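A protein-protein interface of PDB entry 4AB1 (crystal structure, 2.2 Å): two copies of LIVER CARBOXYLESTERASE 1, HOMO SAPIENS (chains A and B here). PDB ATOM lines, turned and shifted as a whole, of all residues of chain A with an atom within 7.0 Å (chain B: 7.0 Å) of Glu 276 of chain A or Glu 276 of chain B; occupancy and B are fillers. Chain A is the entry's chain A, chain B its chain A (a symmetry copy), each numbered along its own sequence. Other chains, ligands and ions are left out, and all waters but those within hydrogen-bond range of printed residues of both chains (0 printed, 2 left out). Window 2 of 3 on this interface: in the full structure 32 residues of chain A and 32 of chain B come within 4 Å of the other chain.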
ATOM      1  N   ILE A 154     -16.639 -24.674  35.548  1.00  0.00           N
ATOM      2  CA  ILE A 154     -16.001 -25.875  34.954  1.00  0.00           C
ATOM      3  C   ILE A 154     -14.858 -26.411  35.827  1.00  0.00           C
ATOM      4  O   ILE A 154     -14.778 -27.635  36.101  1.00  0.00           O
ATOM      5  CB  ILE A 154     -15.506 -25.598  33.513  1.00  0.00           C
ATOM      6  CG1 ILE A 154     -16.739 -25.346  32.558  1.00  0.00           C
ATOM      7  CG2 ILE A 154     -14.737 -26.814  32.955  1.00  0.00           C
ATOM      8  CD1 ILE A 154     -16.334 -24.768  31.185  1.00  0.00           C
ATOM      9  N   TRP A 155     -14.016 -25.488  36.292  1.00  0.00           N
ATOM     10  CA  TRP A 155     -12.834 -25.848  37.086  1.00  0.00           C
ATOM     11  C   TRP A 155     -13.286 -26.554  38.359  1.00  0.00           C
ATOM     12  O   TRP A 155     -12.602 -27.455  38.877  1.00  0.00           O
ATOM     13  CB  TRP A 155     -12.007 -24.596  37.430  1.00  0.00           C
ATOM     14  CG  TRP A 155     -11.475 -23.836  36.209  1.00  0.00           C
ATOM     15  CD1 TRP A 155     -10.181 -23.928  35.635  1.00  0.00           C
ATOM     16  CD2 TRP A 155     -12.181 -22.845  35.389  1.00  0.00           C
ATOM     17  NE1 TRP A 155     -10.054 -23.088  34.550  1.00  0.00           N
ATOM     18  CE2 TRP A 155     -11.217 -22.395  34.352  1.00  0.00           C
ATOM     19  CE3 TRP A 155     -13.473 -22.320  35.386  1.00  0.00           C
ATOM     20  CZ2 TRP A 155     -11.576 -21.495  33.356  1.00  0.00           C
ATOM     21  CZ3 TRP A 155     -13.806 -21.387  34.399  1.00  0.00           C
ATOM     22  CH2 TRP A 155     -12.889 -21.017  33.401  1.00  0.00           C
ATOM     23  N   THR A 251     -18.561 -27.948  23.092  1.00  0.00           N
ATOM     24  CA  THR A 251     -18.426 -26.508  23.024  1.00  0.00           C
ATOM     25  C   THR A 251     -16.976 -26.073  23.053  1.00  0.00           C
ATOM     26  O   THR A 251     -16.610 -25.069  22.428  1.00  0.00           O
ATOM     27  CB  THR A 251     -19.192 -25.841  24.160  1.00  0.00           C
ATOM     28  OG1 THR A 251     -20.536 -26.318  24.085  1.00  0.00           O
ATOM     29  CG2 THR A 251     -19.205 -24.351  23.955  1.00  0.00           C
ATOM     30  N   THR A 270      -6.382 -23.834  27.585  1.00  0.00           N
ATOM     31  CA  THR A 270      -5.860 -22.756  28.435  1.00  0.00           C
ATOM     32  C   THR A 270      -7.068 -22.268  29.289  1.00  0.00           C
ATOM     33  O   THR A 270      -8.262 -22.549  28.954  1.00  0.00           O
ATOM     34  CB  THR A 270      -5.299 -21.554  27.604  1.00  0.00           C
ATOM     35  OG1 THR A 270      -6.384 -20.974  26.923  1.00  0.00           O
ATOM     36  CG2 THR A 270      -4.167 -21.990  26.526  1.00  0.00           C
ATOM     37  N   GLU A 271      -6.742 -21.516  30.341  1.00  0.00           N
ATOM     38  CA  GLU A 271      -7.723 -20.791  31.158  1.00  0.00           C
ATOM     39  C   GLU A 271      -8.682 -19.996  30.249  1.00  0.00           C
ATOM     40  O   GLU A 271      -9.950 -20.120  30.302  1.00  0.00           O
ATOM     41  CB  GLU A 271      -6.969 -19.857  32.141  1.00  0.00           C
ATOM     42  CG  GLU A 271      -7.979 -19.057  33.015  1.00  0.00           C
ATOM     43  CD  GLU A 271      -7.345 -18.004  33.945  1.00  0.00           C
ATOM     44  OE1 GLU A 271      -6.181 -17.547  33.724  1.00  0.00           O
ATOM     45  OE2 GLU A 271      -8.004 -17.650  34.963  1.00  0.00           O
ATOM     46  N   GLU A 272      -8.102 -19.203  29.356  1.00  0.00           N
ATOM     47  CA  GLU A 272      -8.923 -18.446  28.402  1.00  0.00           C
ATOM     48  C   GLU A 272      -9.838 -19.314  27.570  1.00  0.00           C
ATOM     49  O   GLU A 272     -11.002 -18.954  27.351  1.00  0.00           O
ATOM     50  CB  GLU A 272      -8.033 -17.579  27.487  1.00  0.00           C
ATOM     51  CG  GLU A 272      -8.837 -16.737  26.505  1.00  0.00           C
ATOM     52  CD  GLU A 272      -7.996 -15.712  25.749  1.00  0.00           C
ATOM     53  OE1 GLU A 272      -7.150 -16.094  24.941  1.00  0.00           O
ATOM     54  OE2 GLU A 272      -8.199 -14.507  25.959  1.00  0.00           O
ATOM     55  N   GLU A 273      -9.372 -20.430  27.045  1.00  0.00           N
ATOM     56  CA  GLU A 273     -10.297 -21.261  26.232  1.00  0.00           C
ATOM     57  C   GLU A 273     -11.474 -21.782  27.063  1.00  0.00           C
ATOM     58  O   GLU A 273     -12.595 -21.860  26.556  1.00  0.00           O
ATOM     59  CB  GLU A 273      -9.562 -22.490  25.592  1.00  0.00           C
ATOM     60  CG  GLU A 273      -8.646 -21.997  24.483  1.00  0.00           C
ATOM     61  CD  GLU A 273      -7.588 -22.958  24.000  1.00  0.00           C
ATOM     62  OE1 GLU A 273      -6.972 -23.753  24.745  1.00  0.00           O
ATOM     63  OE2 GLU A 273      -7.329 -22.852  22.801  1.00  0.00           O
ATOM     64  N   LEU A 274     -11.188 -22.192  28.311  1.00  0.00           N
ATOM     65  CA  LEU A 274     -12.220 -22.641  29.208  1.00  0.00           C
ATOM     66  C   LEU A 274     -13.198 -21.516  29.606  1.00  0.00           C
ATOM     67  O   LEU A 274     -14.399 -21.771  29.737  1.00  0.00           O
ATOM     68  CB  LEU A 274     -11.604 -23.347  30.451  1.00  0.00           C
ATOM     69  CG  LEU A 274     -10.976 -24.719  30.127  1.00  0.00           C
ATOM     70  CD1 LEU A 274     -10.583 -25.369  31.415  1.00  0.00           C
ATOM     71  CD2 LEU A 274     -11.923 -25.646  29.353  1.00  0.00           C
ATOM     72  N   LEU A 275     -12.697 -20.294  29.770  1.00  0.00           N
ATOM     73  CA  LEU A 275     -13.575 -19.146  30.010  1.00  0.00           C
ATOM     74  C   LEU A 275     -14.479 -18.836  28.766  1.00  0.00           C
ATOM     75  O   LEU A 275     -15.669 -18.542  28.879  1.00  0.00           O
ATOM     76  CB  LEU A 275     -12.724 -17.900  30.434  1.00  0.00           C
ATOM     77  CG  LEU A 275     -13.563 -16.735  30.939  1.00  0.00           C
ATOM     78  CD1 LEU A 275     -14.544 -17.184  32.056  1.00  0.00           C
ATOM     79  CD2 LEU A 275     -12.685 -15.537  31.336  1.00  0.00           C
ATOM     80  N   GLU A 276     -13.915 -18.971  27.577  1.00  0.00           N
ATOM     81  CA  GLU A 276     -14.689 -18.837  26.343  1.00  0.00           C
ATOM     82  C   GLU A 276     -15.782 -19.896  26.225  1.00  0.00           C
ATOM     83  O   GLU A 276     -16.914 -19.555  25.888  1.00  0.00           O
ATOM     84  CB  GLU A 276     -13.763 -18.867  25.108  1.00  0.00           C
ATOM     85  CG  GLU A 276     -12.967 -17.573  25.036  1.00  0.00           C
ATOM     86  CD  GLU A 276     -11.743 -17.632  24.118  1.00  0.00           C
ATOM     87  OE1 GLU A 276     -11.379 -18.698  23.575  1.00  0.00           O
ATOM     88  OE2 GLU A 276     -11.141 -16.569  23.946  1.00  0.00           O
ATOM     89  N   THR A 277     -15.434 -21.161  26.529  1.00  0.00           N
ATOM     90  CA  THR A 277     -16.456 -22.227  26.665  1.00  0.00           C
ATOM     91  C   THR A 277     -17.553 -21.864  27.667  1.00  0.00           C
ATOM     92  O   THR A 277     -18.719 -21.992  27.340  1.00  0.00           O
ATOM     93  CB  THR A 277     -15.852 -23.588  27.038  1.00  0.00           C
ATOM     94  OG1 THR A 277     -14.813 -23.865  26.106  1.00  0.00           O
ATOM     95  CG2 THR A 277     -16.916 -24.716  26.986  1.00  0.00           C
ATOM     96  N   THR A 278     -17.171 -21.382  28.849  1.00  0.00           N
ATOM     97  CA  THR A 278     -18.155 -20.968  29.843  1.00  0.00           C
ATOM     98  C   THR A 278     -19.083 -19.929  29.259  1.00  0.00           C
ATOM     99  O   THR A 278     -20.312 -20.009  29.396  1.00  0.00           O
ATOM    100  CB  THR A 278     -17.428 -20.375  31.044  1.00  0.00           C
ATOM    101  OG1 THR A 278     -16.534 -21.365  31.573  1.00  0.00           O
ATOM    102  CG2 THR A 278     -18.440 -19.913  32.135  1.00  0.00           C
ATOM    103  N   LEU A 279     -18.489 -18.971  28.545  1.00  0.00           N
ATOM    104  CA  LEU A 279     -19.243 -17.837  27.990  1.00  0.00           C
ATOM    105  C   LEU A 279     -20.261 -18.350  26.956  1.00  0.00           C
ATOM    106  O   LEU A 279     -21.433 -18.010  27.025  1.00  0.00           O
ATOM    107  CB  LEU A 279     -18.274 -16.712  27.514  1.00  0.00           C
ATOM    108  CG  LEU A 279     -17.958 -15.581  28.565  1.00  0.00           C
ATOM    109  CD1 LEU A 279     -17.832 -15.923  30.073  1.00  0.00           C
ATOM    110  CD2 LEU A 279     -16.835 -14.598  28.173  1.00  0.00           C
ATOM    111  N   LYS A 280     -19.845 -19.297  26.126  1.00  0.00           N
ATOM    112  CA  LYS A 280     -20.721 -19.886  25.131  1.00  0.00           C
ATOM    113  C   LYS A 280     -21.830 -20.741  25.677  1.00  0.00           C
ATOM    114  O   LYS A 280     -22.866 -20.911  25.003  1.00  0.00           O
ATOM    115  CB  LYS A 280     -19.905 -20.747  24.142  1.00  0.00           C
ATOM    116  CG  LYS A 280     -19.045 -19.890  23.228  1.00  0.00           C
ATOM    117  CD  LYS A 280     -18.188 -20.771  22.297  1.00  0.00           C
ATOM    118  CE  LYS A 280     -17.014 -19.996  21.786  1.00  0.00           C
ATOM    119  NZ  LYS A 280     -16.189 -20.978  21.015  1.00  0.00           N
ATOM    120  N   MET A 281     -21.642 -21.331  26.864  1.00  0.00           N
ATOM    121  CA  MET A 281     -22.761 -22.088  27.437  1.00  0.00           C
ATOM    122  C   MET A 281     -23.884 -21.190  28.036  1.00  0.00           C
ATOM    123  O   MET A 281     -24.973 -21.683  28.302  1.00  0.00           O
ATOM    124  CB  MET A 281     -22.265 -23.053  28.494  1.00  0.00           C
ATOM    125  CG  MET A 281     -21.074 -23.899  28.079  1.00  0.00           C
ATOM    126  SD  MET A 281     -21.613 -25.452  27.428  1.00  0.00           S
ATOM    127  CE  MET A 281     -23.061 -25.830  28.406  1.00  0.00           C
ATOM    128  N   ILE B 154     -19.897  -6.819  14.131  1.00  0.00           N
ATOM    129  CA  ILE B 154     -18.518  -6.444  13.731  1.00  0.00           C
ATOM    130  C   ILE B 154     -18.341  -6.450  12.205  1.00  0.00           C
ATOM    131  O   ILE B 154     -17.788  -5.483  11.620  1.00  0.00           O
ATOM    132  CB  ILE B 154     -17.465  -7.356  14.407  1.00  0.00           C
ATOM    133  CG1 ILE B 154     -17.458  -7.105  15.967  1.00  0.00           C
ATOM    134  CG2 ILE B 154     -16.048  -7.034  13.887  1.00  0.00           C
ATOM    135  CD1 ILE B 154     -16.664  -8.174  16.749  1.00  0.00           C
ATOM    136  N   TRP B 155     -18.849  -7.508  11.576  1.00  0.00           N
ATOM    137  CA  TRP B 155     -18.702  -7.693  10.126  1.00  0.00           C
ATOM    138  C   TRP B 155     -19.371  -6.527   9.406  1.00  0.00           C
ATOM    139  O   TRP B 155     -18.926  -6.089   8.331  1.00  0.00           O
ATOM    140  CB  TRP B 155     -19.324  -9.028   9.681  1.00  0.00           C
ATOM    141  CG  TRP B 155     -18.688 -10.266  10.327  1.00  0.00           C
ATOM    142  CD1 TRP B 155     -17.694 -11.111   9.771  1.00  0.00           C
ATOM    143  CD2 TRP B 155     -18.984 -10.846  11.641  1.00  0.00           C
ATOM    144  NE1 TRP B 155     -17.369 -12.136  10.634  1.00  0.00           N
ATOM    145  CE2 TRP B 155     -18.119 -12.046  11.775  1.00  0.00           C
ATOM    146  CE3 TRP B 155     -19.827 -10.499  12.697  1.00  0.00           C
ATOM    147  CZ2 TRP B 155     -18.094 -12.809  12.936  1.00  0.00           C
ATOM    148  CZ3 TRP B 155     -19.817 -11.300  13.843  1.00  0.00           C
ATOM    149  CH2 TRP B 155     -18.952 -12.399  13.961  1.00  0.00           C
ATOM    150  N   THR B 251     -10.091  -6.773  22.697  1.00  0.00           N
ATOM    151  CA  THR B 251     -10.822  -7.968  23.060  1.00  0.00           C
ATOM    152  C   THR B 251     -10.489  -9.133  22.152  1.00  0.00           C
ATOM    153  O   THR B 251     -10.482 -10.290  22.593  1.00  0.00           O
ATOM    154  CB  THR B 251     -12.323  -7.708  23.043  1.00  0.00           C
ATOM    155  OG1 THR B 251     -12.555  -6.586  23.895  1.00  0.00           O
ATOM    156  CG2 THR B 251     -13.050  -8.896  23.612  1.00  0.00           C
ATOM    157  N   THR B 270     -10.533 -15.690  12.415  1.00  0.00           N
ATOM    158  CA  THR B 270     -11.534 -16.572  11.801  1.00  0.00           C
ATOM    159  C   THR B 270     -12.918 -15.999  12.227  1.00  0.00           C
ATOM    160  O   THR B 270     -13.020 -15.188  13.200  1.00  0.00           O
ATOM    161  CB  THR B 270     -11.415 -18.051  12.298  1.00  0.00           C
ATOM    162  OG1 THR B 270     -11.729 -18.059  13.669  1.00  0.00           O
ATOM    163  CG2 THR B 270      -9.936 -18.685  12.088  1.00  0.00           C
ATOM    164  N   GLU B 271     -13.955 -16.460  11.525  1.00  0.00           N
ATOM    165  CA  GLU B 271     -15.356 -16.209  11.883  1.00  0.00           C
ATOM    166  C   GLU B 271     -15.581 -16.521  13.376  1.00  0.00           C
ATOM    167  O   GLU B 271     -16.076 -15.675  14.193  1.00  0.00           O
ATOM    168  CB  GLU B 271     -16.270 -17.078  10.979  1.00  0.00           C
ATOM    169  CG  GLU B 271     -17.768 -16.852  11.342  1.00  0.00           C
ATOM    170  CD  GLU B 271     -18.764 -17.757  10.590  1.00  0.00           C
ATOM    171  OE1 GLU B 271     -18.388 -18.844  10.053  1.00  0.00           O
ATOM    172  OE2 GLU B 271     -19.956 -17.354  10.486  1.00  0.00           O
ATOM    173  N   GLU B 272     -15.175 -17.717  13.783  1.00  0.00           N
ATOM    174  CA  GLU B 272     -15.291 -18.091  15.199  1.00  0.00           C
ATOM    175  C   GLU B 272     -14.588 -17.137  16.135  1.00  0.00           C
ATOM    176  O   GLU B 272     -15.130 -16.798  17.196  1.00  0.00           O
ATOM    177  CB  GLU B 272     -14.782 -19.531  15.424  1.00  0.00           C
ATOM    178  CG  GLU B 272     -14.919 -19.988  16.870  1.00  0.00           C
ATOM    179  CD  GLU B 272     -14.634 -21.473  17.071  1.00  0.00           C
ATOM    180  OE1 GLU B 272     -13.494 -21.904  16.899  1.00  0.00           O
ATOM    181  OE2 GLU B 272     -15.564 -22.214  17.420  1.00  0.00           O
ATOM    182  N   GLU B 273     -13.378 -16.706  15.833  1.00  0.00           N
ATOM    183  CA  GLU B 273     -12.713 -15.768  16.776  1.00  0.00           C
ATOM    184  C   GLU B 273     -13.484 -14.450  16.906  1.00  0.00           C
ATOM    185  O   GLU B 273     -13.553 -13.886  17.999  1.00  0.00           O
ATOM    186  CB  GLU B 273     -11.247 -15.440  16.329  1.00  0.00           C
ATOM    187  CG  GLU B 273     -10.375 -16.665  16.557  1.00  0.00           C
ATOM    188  CD  GLU B 273      -9.037 -16.685  15.858  1.00  0.00           C
ATOM    189  OE1 GLU B 273      -8.840 -16.223  14.711  1.00  0.00           O
ATOM    190  OE2 GLU B 273      -8.151 -17.259  16.492  1.00  0.00           O
ATOM    191  N   LEU B 274     -14.000 -13.946  15.770  1.00  0.00           N
ATOM    192  CA  LEU B 274     -14.797 -12.748  15.776  1.00  0.00           C
ATOM    193  C   LEU B 274     -16.138 -12.925  16.521  1.00  0.00           C
ATOM    194  O   LEU B 274     -16.582 -11.996  17.202  1.00  0.00           O
ATOM    195  CB  LEU B 274     -14.999 -12.211  14.329  1.00  0.00           C
ATOM    196  CG  LEU B 274     -13.715 -11.622  13.709  1.00  0.00           C
ATOM    197  CD1 LEU B 274     -14.075 -10.987  12.405  1.00  0.00           C
ATOM    198  CD2 LEU B 274     -13.031 -10.588  14.613  1.00  0.00           C
ATOM    199  N   LEU B 275     -16.752 -14.100  16.413  1.00  0.00           N
ATOM    200  CA  LEU B 275     -17.952 -14.398  17.199  1.00  0.00           C
ATOM    201  C   LEU B 275     -17.639 -14.466  18.734  1.00  0.00           C
ATOM    202  O   LEU B 275     -18.386 -13.967  19.576  1.00  0.00           O
ATOM    203  CB  LEU B 275     -18.615 -15.720  16.682  1.00  0.00           C
ATOM    204  CG  LEU B 275     -19.995 -15.978  17.271  1.00  0.00           C
ATOM    205  CD1 LEU B 275     -20.925 -14.747  17.097  1.00  0.00           C
ATOM    206  CD2 LEU B 275     -20.601 -17.287  16.740  1.00  0.00           C
ATOM    207  N   GLU B 276     -16.494 -15.031  19.080  1.00  0.00           N
ATOM    208  CA  GLU B 276     -16.032 -15.037  20.468  1.00  0.00           C
ATOM    209  C   GLU B 276     -15.792 -13.629  21.006  1.00  0.00           C
ATOM    210  O   GLU B 276     -16.227 -13.329  22.116  1.00  0.00           O
ATOM    211  CB  GLU B 276     -14.764 -15.904  20.620  1.00  0.00           C
ATOM    212  CG  GLU B 276     -15.132 -17.374  20.481  1.00  0.00           C
ATOM    213  CD  GLU B 276     -13.945 -18.302  20.210  1.00  0.00           C
ATOM    214  OE1 GLU B 276     -12.795 -17.856  20.006  1.00  0.00           O
ATOM    215  OE2 GLU B 276     -14.190 -19.511  20.206  1.00  0.00           O
ATOM    216  N   THR B 277     -15.125 -12.779  20.202  1.00  0.00           N
ATOM    217  CA  THR B 277     -15.029 -11.334  20.522  1.00  0.00           C
ATOM    218  C   THR B 277     -16.397 -10.688  20.736  1.00  0.00           C
ATOM    219  O   THR B 277     -16.583 -10.008  21.730  1.00  0.00           O
ATOM    220  CB  THR B 277     -14.248 -10.540  19.466  1.00  0.00           C
ATOM    221  OG1 THR B 277     -13.001 -11.198  19.270  1.00  0.00           O
ATOM    222  CG2 THR B 277     -14.002  -9.078  19.921  1.00  0.00           C
ATOM    223  N   THR B 278     -17.345 -10.939  19.834  1.00  0.00           N
ATOM    224  CA  THR B 278     -18.691 -10.400  19.989  1.00  0.00           C
ATOM    225  C   THR B 278     -19.273 -10.820  21.317  1.00  0.00           C
ATOM    226  O   THR B 278     -19.836 -10.008  22.064  1.00  0.00           O
ATOM    227  CB  THR B 278     -19.571 -10.930  18.863  1.00  0.00           C
ATOM    228  OG1 THR B 278     -18.994 -10.542  17.608  1.00  0.00           O
ATOM    229  CG2 THR B 278     -21.025 -10.383  18.989  1.00  0.00           C
ATOM    230  N   LEU B 279     -19.081 -12.100  21.644  1.00  0.00           N
ATOM    231  CA  LEU B 279     -19.666 -12.686  22.860  1.00  0.00           C
ATOM    232  C   LEU B 279     -19.070 -12.001  24.102  1.00  0.00           C
ATOM    233  O   LEU B 279     -19.805 -11.560  24.974  1.00  0.00           O
ATOM    234  CB  LEU B 279     -19.581 -14.243  22.815  1.00  0.00           C
ATOM    235  CG  LEU B 279     -20.840 -14.987  22.230  1.00  0.00           C
ATOM    236  CD1 LEU B 279     -21.644 -14.369  21.056  1.00  0.00           C
ATOM    237  CD2 LEU B 279     -20.667 -16.501  21.982  1.00  0.00           C
ATOM    238  N   LYS B 280     -17.767 -11.757  24.084  1.00  0.00           N
ATOM    239  CA  LYS B 280     -17.095 -11.085  25.179  1.00  0.00           C
ATOM    240  C   LYS B 280     -17.444  -9.633  25.352  1.00  0.00           C
ATOM    241  O   LYS B 280     -17.307  -9.095  26.470  1.00  0.00           O
ATOM    242  CB  LYS B 280     -15.563 -11.184  25.010  1.00  0.00           C
ATOM    243  CG  LYS B 280     -15.062 -12.598  25.253  1.00  0.00           C
ATOM    244  CD  LYS B 280     -13.542 -12.690  25.012  1.00  0.00           C
ATOM    245  CE  LYS B 280     -13.145 -14.108  24.747  1.00  0.00           C
ATOM    246  NZ  LYS B 280     -11.691 -14.059  24.394  1.00  0.00           N
ATOM    247  N   MET B 281     -17.854  -8.952  24.275  1.00  0.00           N
ATOM    248  CA  MET B 281     -18.283  -7.561  24.466  1.00  0.00           C
ATOM    249  C   MET B 281     -19.691  -7.424  25.115  1.00  0.00           C
ATOM    250  O   MET B 281     -20.046  -6.340  25.561  1.00  0.00           O
ATOM    251  CB  MET B 281     -18.255  -6.811  23.150  1.00  0.00           C
ATOM    252  CG  MET B 281     -16.976  -6.976  22.346  1.00  0.00           C
ATOM    253  SD  MET B 281     -15.845  -5.665  22.706  1.00  0.00           S
ATOM    254  CE  MET B 281     -16.915  -4.257  22.970  1.00  0.00           C
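The side-chain amino group of Lys 280 of chain A is in salt-bridge range of the side-chain carboxylate of Glu 276 of chain B, at 2.6 Å. OE2 of Glu 272 of chain A lies within salt-bridge range of NZ of Lys 280 of chain B (3.9 Å). NZ of Lys 280 of chain B is in salt-bridge range of OE2 of Glu 276 of chain A. The side-chain carboxylate of Glu 272 of chain B is in salt-bridge range of the side-chain amino group of Lys 280 of chain A, 3.9 Å away.
The side-chain hydroxyl of Thr 270 of chain B lies close to the backbone NH of Glu 272 of chain B, 3.5 Å away. N of Glu 272 of chain A lies close to OG1 of Thr 270 of chain A (3.5 Å).
Glu 276 of chain A touches Glu 276 of chain B (OE1 to OE1, 3.9 Å). Lys 280 of chain B touches Leu 279 of chain A (CG to CD2, 3.96 Å). CD2 of Leu 279 of chain B touches CG of Lys 280 of chain A, 3.96 Å away.
Of chain A, only Glu 276 (3.9 Å) and Lys 280 (2.6 Å) come within 4 Å of Glu 276 of chain B. Printed residues of chain A within 4 Å of Lys 280 of chain B: Glu 272 (3.9 Å), Glu 276 (2.6 Å) and Leu 279 (3.96 Å). Of the printed residues of chain A, Leu 279 of chain B touches Lys 280. Printed residues of chain A within 4 Å of Glu 272 of chain B: Lys 280. Of the printed residues of chain B, Lys 280 of chain A touches Glu 272, Glu 276 and Leu 279.
Of the 15 printed residues of chain A, 4 touch a printed residue of chain B. Of the 15 printed residues of chain B, 4 touch a printed residue of chain A.
Glu 272 of chain A touches Lys 280 of chain B, and with the chains exchanged Lys 280 of chain A touches Glu 272 of chain B. Glu 276 of chain B touches its own counterpart, Glu 276 of chain A. Glu 276 of chain A touches Lys 280 of chain B, and with the chains exchanged Lys 280 of chain A touches Glu 276 of chain B. Leu 279 of chain A touches Lys 280 of chain B, and with the chains exchanged Lys 280 of chain A touches Leu 279 of chain B. Of the 7 pairs that touch across the chains among the printed residues, 7 have their exchanged pair printed and touching as well.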
